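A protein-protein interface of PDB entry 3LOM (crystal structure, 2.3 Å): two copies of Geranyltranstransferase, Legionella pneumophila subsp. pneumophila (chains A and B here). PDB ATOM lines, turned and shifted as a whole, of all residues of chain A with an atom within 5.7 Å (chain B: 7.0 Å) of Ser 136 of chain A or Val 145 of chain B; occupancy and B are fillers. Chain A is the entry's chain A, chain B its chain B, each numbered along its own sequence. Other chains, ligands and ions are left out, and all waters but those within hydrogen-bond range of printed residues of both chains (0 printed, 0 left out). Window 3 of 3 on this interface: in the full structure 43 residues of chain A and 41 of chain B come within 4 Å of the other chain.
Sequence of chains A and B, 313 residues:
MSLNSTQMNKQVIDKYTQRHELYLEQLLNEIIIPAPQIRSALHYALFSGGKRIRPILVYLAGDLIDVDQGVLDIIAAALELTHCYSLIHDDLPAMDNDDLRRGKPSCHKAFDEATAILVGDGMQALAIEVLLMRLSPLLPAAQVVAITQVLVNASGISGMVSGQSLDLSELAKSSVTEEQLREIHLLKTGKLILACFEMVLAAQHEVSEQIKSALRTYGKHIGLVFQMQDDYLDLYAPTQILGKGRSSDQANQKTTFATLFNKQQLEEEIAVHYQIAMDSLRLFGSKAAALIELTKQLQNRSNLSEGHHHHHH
O of Val 144 of chain B lies within hydrogen-bond range of OG1 of Thr 148 of chain B, at 2.7 Å.
The side-chain hydroxyl (OG) of Ser 136 of chain A lies within hydrogen-bond range of the backbone carbonyl oxygen (O) of Leu 132 of chain A.
Among the printed residues, merely in contact across the chains: Leu 132 of chain A with Val 145 of chain B, Leu 132 of chain A with Thr 148 of chain B, Leu 132 of chain A with Gln 149 of chain B, Met 133 of chain A with Gln 149 of chain B, Ser 136 of chain A with Val 145 of chain B, Ala 141 of chain A with Ala 141 of chain B, Ala 141 of chain A with Ala 142 of chain B, Val 144 of chain A with Val 145 of chain B, Val 145 of chain A with Leu 132 of chain B, Val 145 of chain A with Ala 141 of chain B and Val 145 of chain A with Val 145 of chain B.
Ser 136 of chain A touches one residue of chain B.
Of the printed residues of chain B, Ala 141 of chain A touches Ala 141 and Ala 142.
Printed residues of chain A within 4 Å of Ala 141 of chain B: Ala 141 and Val 145.
Of the printed residues of chain B, Leu 132 of chain A touches Val 145 (3.9 Å), Thr 148 (3.7 Å) and Gln 149 (3.5 Å).
Of the printed residues of chain B, Val 145 of chain A touches Leu 132 (3.9 Å), Ala 141 (3.9 Å) and Val 145 (3.8 Å).
Ile 147 of chain B touches none of the printed residues of chain A.
The nearest residue of chain B that does not touch Ser 136 of chain A is Gln 149 of chain B (6.4 Å).
The nearest printed residue of chain A that does not touch Gln 149 of chain B is Arg 134 of chain A (6.2 Å).
Hydrophobic or aromatic side chains of chain B that line the printed part of chain A: Leu 132, Ala 141 and Val 145.
Printed residues of chain A that touch a printed residue of chain B: Leu 132, Met 133, Ser 136, Ala 141, Val 144 and Val 145.
Hydrophobic or aromatic side chains of chain A that line the printed part of chain B: Leu 132, Met 133, Ala 141, Val 144 and Val 145.
Ala 141 of chain A touches its own counterpart, Ala 141 of chain B.
Val 144 of chain A touches Val 145 of chain B, but with the chains exchanged Val 145 of chain A does not touch Val 144 of chain B (4.1 Å).
Val 145 of chain A touches Ala 141 of chain B, but with the chains exchanged Ala 141 of chain A does not touch Val 145 of chain B (4.1 Å).
Val 145 of chain B touches its own counterpart, Val 145 of chain A.
Positions printed for both chains: 132, 141, 144 and 145.
Of the 11 pairs that touch across the chains among the printed residues, 4 have their exchanged pair printed and touching as well.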
ATOM      1  N   LEU A 131     -14.939   8.845 -17.872  1.00  0.00           N
ATOM      2  CA  LEU A 131     -14.051   8.109 -16.972  1.00  0.00           C
ATOM      3  C   LEU A 131     -12.998   7.348 -17.754  1.00  0.00           C
ATOM      4  O   LEU A 131     -11.814   7.499 -17.494  1.00  0.00           O
ATOM      5  CB  LEU A 131     -14.822   7.147 -16.069  1.00  0.00           C
ATOM      6  CG  LEU A 131     -15.638   7.731 -14.916  1.00  0.00           C
ATOM      7  CD1 LEU A 131     -16.520   6.654 -14.314  1.00  0.00           C
ATOM      8  CD2 LEU A 131     -14.774   8.384 -13.852  1.00  0.00           C
ATOM      9  N   LEU A 132     -13.434   6.566 -18.736  1.00  0.00           N
ATOM     10  CA  LEU A 132     -12.524   5.734 -19.513  1.00  0.00           C
ATOM     11  C   LEU A 132     -11.495   6.463 -20.387  1.00  0.00           C
ATOM     12  O   LEU A 132     -10.322   6.089 -20.359  1.00  0.00           O
ATOM     13  CB  LEU A 132     -13.298   4.728 -20.358  1.00  0.00           C
ATOM     14  CG  LEU A 132     -14.169   3.698 -19.637  1.00  0.00           C
ATOM     15  CD1 LEU A 132     -14.766   2.791 -20.683  1.00  0.00           C
ATOM     16  CD2 LEU A 132     -13.407   2.902 -18.567  1.00  0.00           C
ATOM     17  N   MET A 133     -11.905   7.482 -21.151  1.00  0.00           N
ATOM     18  CA  MET A 133     -10.977   8.175 -22.055  1.00  0.00           C
ATOM     19  C   MET A 133     -10.064   9.195 -21.351  1.00  0.00           C
ATOM     20  O   MET A 133      -8.888   9.322 -21.696  1.00  0.00           O
ATOM     21  CB  MET A 133     -11.694   8.777 -23.286  1.00  0.00           C
ATOM     22  CG  MET A 133     -12.625   9.969 -23.033  1.00  0.00           C
ATOM     23  SD  MET A 133     -13.589  10.476 -24.481  1.00  0.00           S
ATOM     24  CE  MET A 133     -14.589  11.780 -23.754  1.00  0.00           C
ATOM     25  N   ARG A 134     -10.608   9.909 -20.361  1.00  0.00           N
ATOM     26  CA  ARG A 134      -9.863  10.982 -19.685  1.00  0.00           C
ATOM     27  C   ARG A 134      -8.943  10.537 -18.542  1.00  0.00           C
ATOM     28  O   ARG A 134      -7.930  11.192 -18.285  1.00  0.00           O
ATOM     29  CB  ARG A 134     -10.797  12.104 -19.205  1.00  0.00           C
ATOM     30  CG  ARG A 134     -11.609  12.782 -20.304  1.00  0.00           C
ATOM     31  CD  ARG A 134     -10.739  13.655 -21.200  1.00  0.00           C
ATOM     32  NE  ARG A 134     -11.484  14.202 -22.331  1.00  0.00           N
ATOM     33  CZ  ARG A 134     -12.146  15.357 -22.314  1.00  0.00           C
ATOM     34  NH1 ARG A 134     -12.170  16.108 -21.216  1.00  0.00           N
ATOM     35  NH2 ARG A 134     -12.791  15.762 -23.399  1.00  0.00           N
ATOM     36  N   LEU A 135      -9.289   9.446 -17.856  1.00  0.00           N
ATOM     37  CA  LEU A 135      -8.442   8.926 -16.769  1.00  0.00           C
ATOM     38  C   LEU A 135      -7.255   8.101 -17.266  1.00  0.00           C
ATOM     39  O   LEU A 135      -6.233   8.021 -16.585  1.00  0.00           O
ATOM     40  CB  LEU A 135      -9.250   8.095 -15.761  1.00  0.00           C
ATOM     41  CG  LEU A 135     -10.229   8.773 -14.798  1.00  0.00           C
ATOM     42  CD1 LEU A 135     -10.983   7.717 -14.009  1.00  0.00           C
ATOM     43  CD2 LEU A 135      -9.536   9.744 -13.860  1.00  0.00           C
ATOM     44  N   SER A 136      -7.406   7.493 -18.442  1.00  0.00           N
ATOM     45  CA  SER A 136      -6.408   6.584 -19.010  1.00  0.00           C
ATOM     46  C   SER A 136      -5.003   7.144 -19.310  1.00  0.00           C
ATOM     47  O   SER A 136      -4.029   6.394 -19.221  1.00  0.00           O
ATOM     48  CB  SER A 136      -6.970   5.884 -20.247  1.00  0.00           C
ATOM     49  OG  SER A 136      -7.943   4.935 -19.864  1.00  0.00           O
ATOM     50  N   PRO A 137      -4.881   8.440 -19.681  1.00  0.00           N
ATOM     51  CA  PRO A 137      -3.491   8.912 -19.727  1.00  0.00           C
ATOM     52  C   PRO A 137      -2.923   9.268 -18.345  1.00  0.00           C
ATOM     53  O   PRO A 137      -1.704   9.370 -18.197  1.00  0.00           O
ATOM     54  CB  PRO A 137      -3.569  10.170 -20.609  1.00  0.00           C
ATOM     55  CG  PRO A 137      -4.911  10.110 -21.284  1.00  0.00           C
ATOM     56  CD  PRO A 137      -5.796   9.414 -20.311  1.00  0.00           C
ATOM     57  N   LEU A 138      -3.794   9.430 -17.349  1.00  0.00           N
ATOM     58  CA  LEU A 138      -3.386   9.934 -16.033  1.00  0.00           C
ATOM     59  C   LEU A 138      -3.154   8.863 -14.958  1.00  0.00           C
ATOM     60  O   LEU A 138      -2.298   9.035 -14.085  1.00  0.00           O
ATOM     61  CB  LEU A 138      -4.393  10.968 -15.519  1.00  0.00           C
ATOM     62  CG  LEU A 138      -4.816  12.117 -16.444  1.00  0.00           C
ATOM     63  CD1 LEU A 138      -5.802  13.023 -15.722  1.00  0.00           C
ATOM     64  CD2 LEU A 138      -3.618  12.927 -16.952  1.00  0.00           C
ATOM     65  N   LEU A 139      -3.916   7.774 -15.019  1.00  0.00           N
ATOM     66  CA  LEU A 139      -3.878   6.723 -14.001  1.00  0.00           C
ATOM     67  C   LEU A 139      -3.590   5.361 -14.635  1.00  0.00           C
ATOM     68  O   LEU A 139      -3.851   5.172 -15.829  1.00  0.00           O
ATOM     69  CB  LEU A 139      -5.213   6.687 -13.244  1.00  0.00           C
ATOM     70  CG  LEU A 139      -5.392   7.317 -11.853  1.00  0.00           C
ATOM     71  CD1 LEU A 139      -4.416   8.441 -11.520  1.00  0.00           C
ATOM     72  CD2 LEU A 139      -6.830   7.784 -11.661  1.00  0.00           C
ATOM     73  N   ALA A 141      -4.353   1.620 -15.737  1.00  0.00           N
ATOM     74  CA  ALA A 141      -5.586   1.071 -16.276  1.00  0.00           C
ATOM     75  C   ALA A 141      -6.419   0.315 -15.233  1.00  0.00           C
ATOM     76  O   ALA A 141      -7.654   0.351 -15.268  1.00  0.00           O
ATOM     77  CB  ALA A 141      -5.268   0.183 -17.461  1.00  0.00           C
ATOM     78  N   VAL A 144      -8.468   2.808 -13.276  1.00  0.00           N
ATOM     79  CA  VAL A 144      -9.541   3.284 -14.156  1.00  0.00           C
ATOM     80  C   VAL A 144     -10.752   2.337 -14.104  1.00  0.00           C
ATOM     81  O   VAL A 144     -11.893   2.780 -13.916  1.00  0.00           O
ATOM     82  CB  VAL A 144      -9.036   3.462 -15.622  1.00  0.00           C
ATOM     83  CG1 VAL A 144     -10.187   3.829 -16.575  1.00  0.00           C
ATOM     84  CG2 VAL A 144      -7.928   4.513 -15.683  1.00  0.00           C
ATOM     85  N   VAL A 145     -10.475   1.039 -14.230  1.00  0.00           N
ATOM     86  CA  VAL A 145     -11.476  -0.019 -14.115  1.00  0.00           C
ATOM     87  C   VAL A 145     -12.185  -0.012 -12.747  1.00  0.00           C
ATOM     88  O   VAL A 145     -13.418   0.009 -12.685  1.00  0.00           O
ATOM     89  CB  VAL A 145     -10.846  -1.395 -14.442  1.00  0.00           C
ATOM     90  CG1 VAL A 145     -11.788  -2.545 -14.107  1.00  0.00           C
ATOM     91  CG2 VAL A 145     -10.456  -1.446 -15.911  1.00  0.00           C
ATOM     92  N   LEU B 132     -16.539  -4.872 -16.857  1.00  0.00           N
ATOM     93  CA  LEU B 132     -15.517  -4.515 -15.888  1.00  0.00           C
ATOM     94  C   LEU B 132     -15.195  -5.610 -14.850  1.00  0.00           C
ATOM     95  O   LEU B 132     -14.021  -5.810 -14.531  1.00  0.00           O
ATOM     96  CB  LEU B 132     -15.882  -3.203 -15.193  1.00  0.00           C
ATOM     97  CG  LEU B 132     -16.095  -1.920 -16.011  1.00  0.00           C
ATOM     98  CD1 LEU B 132     -16.419  -0.804 -15.052  1.00  0.00           C
ATOM     99  CD2 LEU B 132     -14.898  -1.548 -16.893  1.00  0.00           C
ATOM    100  N   PRO B 140      -5.933  -8.118 -19.595  1.00  0.00           N
ATOM    101  CA  PRO B 140      -5.279  -7.013 -18.876  1.00  0.00           C
ATOM    102  C   PRO B 140      -6.182  -5.789 -18.807  1.00  0.00           C
ATOM    103  O   PRO B 140      -7.068  -5.632 -19.638  1.00  0.00           O
ATOM    104  CB  PRO B 140      -4.044  -6.697 -19.729  1.00  0.00           C
ATOM    105  CG  PRO B 140      -3.952  -7.802 -20.751  1.00  0.00           C
ATOM    106  CD  PRO B 140      -5.329  -8.330 -20.925  1.00  0.00           C
ATOM    107  N   ALA B 141      -5.945  -4.934 -17.819  1.00  0.00           N
ATOM    108  CA  ALA B 141      -6.827  -3.814 -17.518  1.00  0.00           C
ATOM    109  C   ALA B 141      -7.006  -2.819 -18.673  1.00  0.00           C
ATOM    110  O   ALA B 141      -8.101  -2.287 -18.864  1.00  0.00           O
ATOM    111  CB  ALA B 141      -6.357  -3.121 -16.276  1.00  0.00           C
ATOM    112  N   ALA B 142      -5.944  -2.604 -19.452  1.00  0.00           N
ATOM    113  CA  ALA B 142      -5.985  -1.740 -20.638  1.00  0.00           C
ATOM    114  C   ALA B 142      -6.907  -2.286 -21.731  1.00  0.00           C
ATOM    115  O   ALA B 142      -7.473  -1.524 -22.522  1.00  0.00           O
ATOM    116  CB  ALA B 142      -4.581  -1.531 -21.188  1.00  0.00           C
ATOM    117  N   GLN B 143      -7.046  -3.608 -21.770  1.00  0.00           N
ATOM    118  CA  GLN B 143      -7.927  -4.266 -22.722  1.00  0.00           C
ATOM    119  C   GLN B 143      -9.376  -4.172 -22.241  1.00  0.00           C
ATOM    120  O   GLN B 143     -10.286  -4.028 -23.047  1.00  0.00           O
ATOM    121  CB  GLN B 143      -7.495  -5.716 -22.919  1.00  0.00           C
ATOM    122  CG  GLN B 143      -7.192  -6.070 -24.360  1.00  0.00           C
ATOM    123  CD  GLN B 143      -5.853  -6.766 -24.531  1.00  0.00           C
ATOM    124  OE1 GLN B 143      -4.882  -6.457 -23.837  1.00  0.00           O
ATOM    125  NE2 GLN B 143      -5.788  -7.699 -25.471  1.00  0.00           N
ATOM    126  N   VAL B 144      -9.576  -4.224 -20.925  1.00  0.00           N
ATOM    127  CA  VAL B 144     -10.900  -4.041 -20.325  1.00  0.00           C
ATOM    128  C   VAL B 144     -11.413  -2.625 -20.622  1.00  0.00           C
ATOM    129  O   VAL B 144     -12.571  -2.455 -21.006  1.00  0.00           O
ATOM    130  CB  VAL B 144     -10.898  -4.323 -18.791  1.00  0.00           C
ATOM    131  CG1 VAL B 144     -12.307  -4.275 -18.222  1.00  0.00           C
ATOM    132  CG2 VAL B 144     -10.268  -5.679 -18.488  1.00  0.00           C
ATOM    133  N   VAL B 145     -10.533  -1.632 -20.475  1.00  0.00           N
ATOM    134  CA  VAL B 145     -10.834  -0.229 -20.786  1.00  0.00           C
ATOM    135  C   VAL B 145     -11.219  -0.047 -22.256  1.00  0.00           C
ATOM    136  O   VAL B 145     -12.268   0.532 -22.560  1.00  0.00           O
ATOM    137  CB  VAL B 145      -9.652   0.709 -20.403  1.00  0.00           C
ATOM    138  CG1 VAL B 145      -9.820   2.112 -21.006  1.00  0.00           C
ATOM    139  CG2 VAL B 145      -9.526   0.805 -18.892  1.00  0.00           C
ATOM    140  N   ALA B 146     -10.389  -0.586 -23.147  1.00  0.00           N
ATOM    141  CA  ALA B 146     -10.567  -0.448 -24.594  1.00  0.00           C
ATOM    142  C   ALA B 146     -11.902  -0.971 -25.108  1.00  0.00           C
ATOM    143  O   ALA B 146     -12.565  -0.295 -25.897  1.00  0.00           O
ATOM    144  CB  ALA B 146      -9.420  -1.119 -25.341  1.00  0.00           C
ATOM    145  N   ILE B 147     -12.304  -2.163 -24.673  1.00  0.00           N
ATOM    146  CA  ILE B 147     -13.538  -2.743 -25.209  1.00  0.00           C
ATOM    147  C   ILE B 147     -14.807  -2.109 -24.593  1.00  0.00           C
ATOM    148  O   ILE B 147     -15.827  -1.990 -25.269  1.00  0.00           O
ATOM    149  CB  ILE B 147     -13.546  -4.310 -25.209  1.00  0.00           C
ATOM    150  CG1 ILE B 147     -14.344  -4.891 -24.056  1.00  0.00           C
ATOM    151  CG2 ILE B 147     -12.152  -4.903 -25.263  1.00  0.00           C
ATOM    152  CD1 ILE B 147     -15.566  -5.556 -24.541  1.00  0.00           C
ATOM    153  N   THR B 148     -14.712  -1.676 -23.335  1.00  0.00           N
ATOM    154  CA  THR B 148     -15.796  -0.959 -22.655  1.00  0.00           C
ATOM    155  C   THR B 148     -15.994   0.429 -23.293  1.00  0.00           C
ATOM    156  O   THR B 148     -17.130   0.899 -23.418  1.00  0.00           O
ATOM    157  CB  THR B 148     -15.540  -0.877 -21.123  1.00  0.00           C
ATOM    158  OG1 THR B 148     -15.197  -2.178 -20.634  1.00  0.00           O
ATOM    159  CG2 THR B 148     -16.766  -0.396 -20.353  1.00  0.00           C
ATOM    160  N   GLN B 149     -14.886   1.047 -23.718  1.00  0.00           N
ATOM    161  CA  GLN B 149     -14.893   2.286 -24.512  1.00  0.00           C
ATOM    162  C   GLN B 149     -15.748   2.177 -25.768  1.00  0.00           C
ATOM    163  O   GLN B 149     -16.609   3.018 -26.003  1.00  0.00           O
ATOM    164  CB  GLN B 149     -13.470   2.688 -24.914  1.00  0.00           C
ATOM    165  CG  GLN B 149     -12.787   3.674 -23.976  1.00  0.00           C
ATOM    166  CD  GLN B 149     -12.897   5.117 -24.446  1.00  0.00           C
ATOM    167  OE1 GLN B 149     -11.889   5.747 -24.775  1.00  0.00           O
ATOM    168  NE2 GLN B 149     -14.119   5.645 -24.482  1.00  0.00           N
ATOM    169  N   VAL B 150     -15.501   1.130 -26.553  1.00  0.00           N
ATOM    170  CA  VAL B 150     -16.242   0.831 -27.781  1.00  0.00           C
ATOM    171  C   VAL B 150     -17.773   0.806 -27.601  1.00  0.00           C
ATOM    172  O   VAL B 150     -18.502   1.415 -28.390  1.00  0.00           O
ATOM    173  CB  VAL B 150     -15.775  -0.517 -28.385  1.00  0.00           C
ATOM    174  CG1 VAL B 150     -16.636  -0.905 -29.563  1.00  0.00           C
ATOM    175  CG2 VAL B 150     -14.307  -0.443 -28.802  1.00  0.00           C
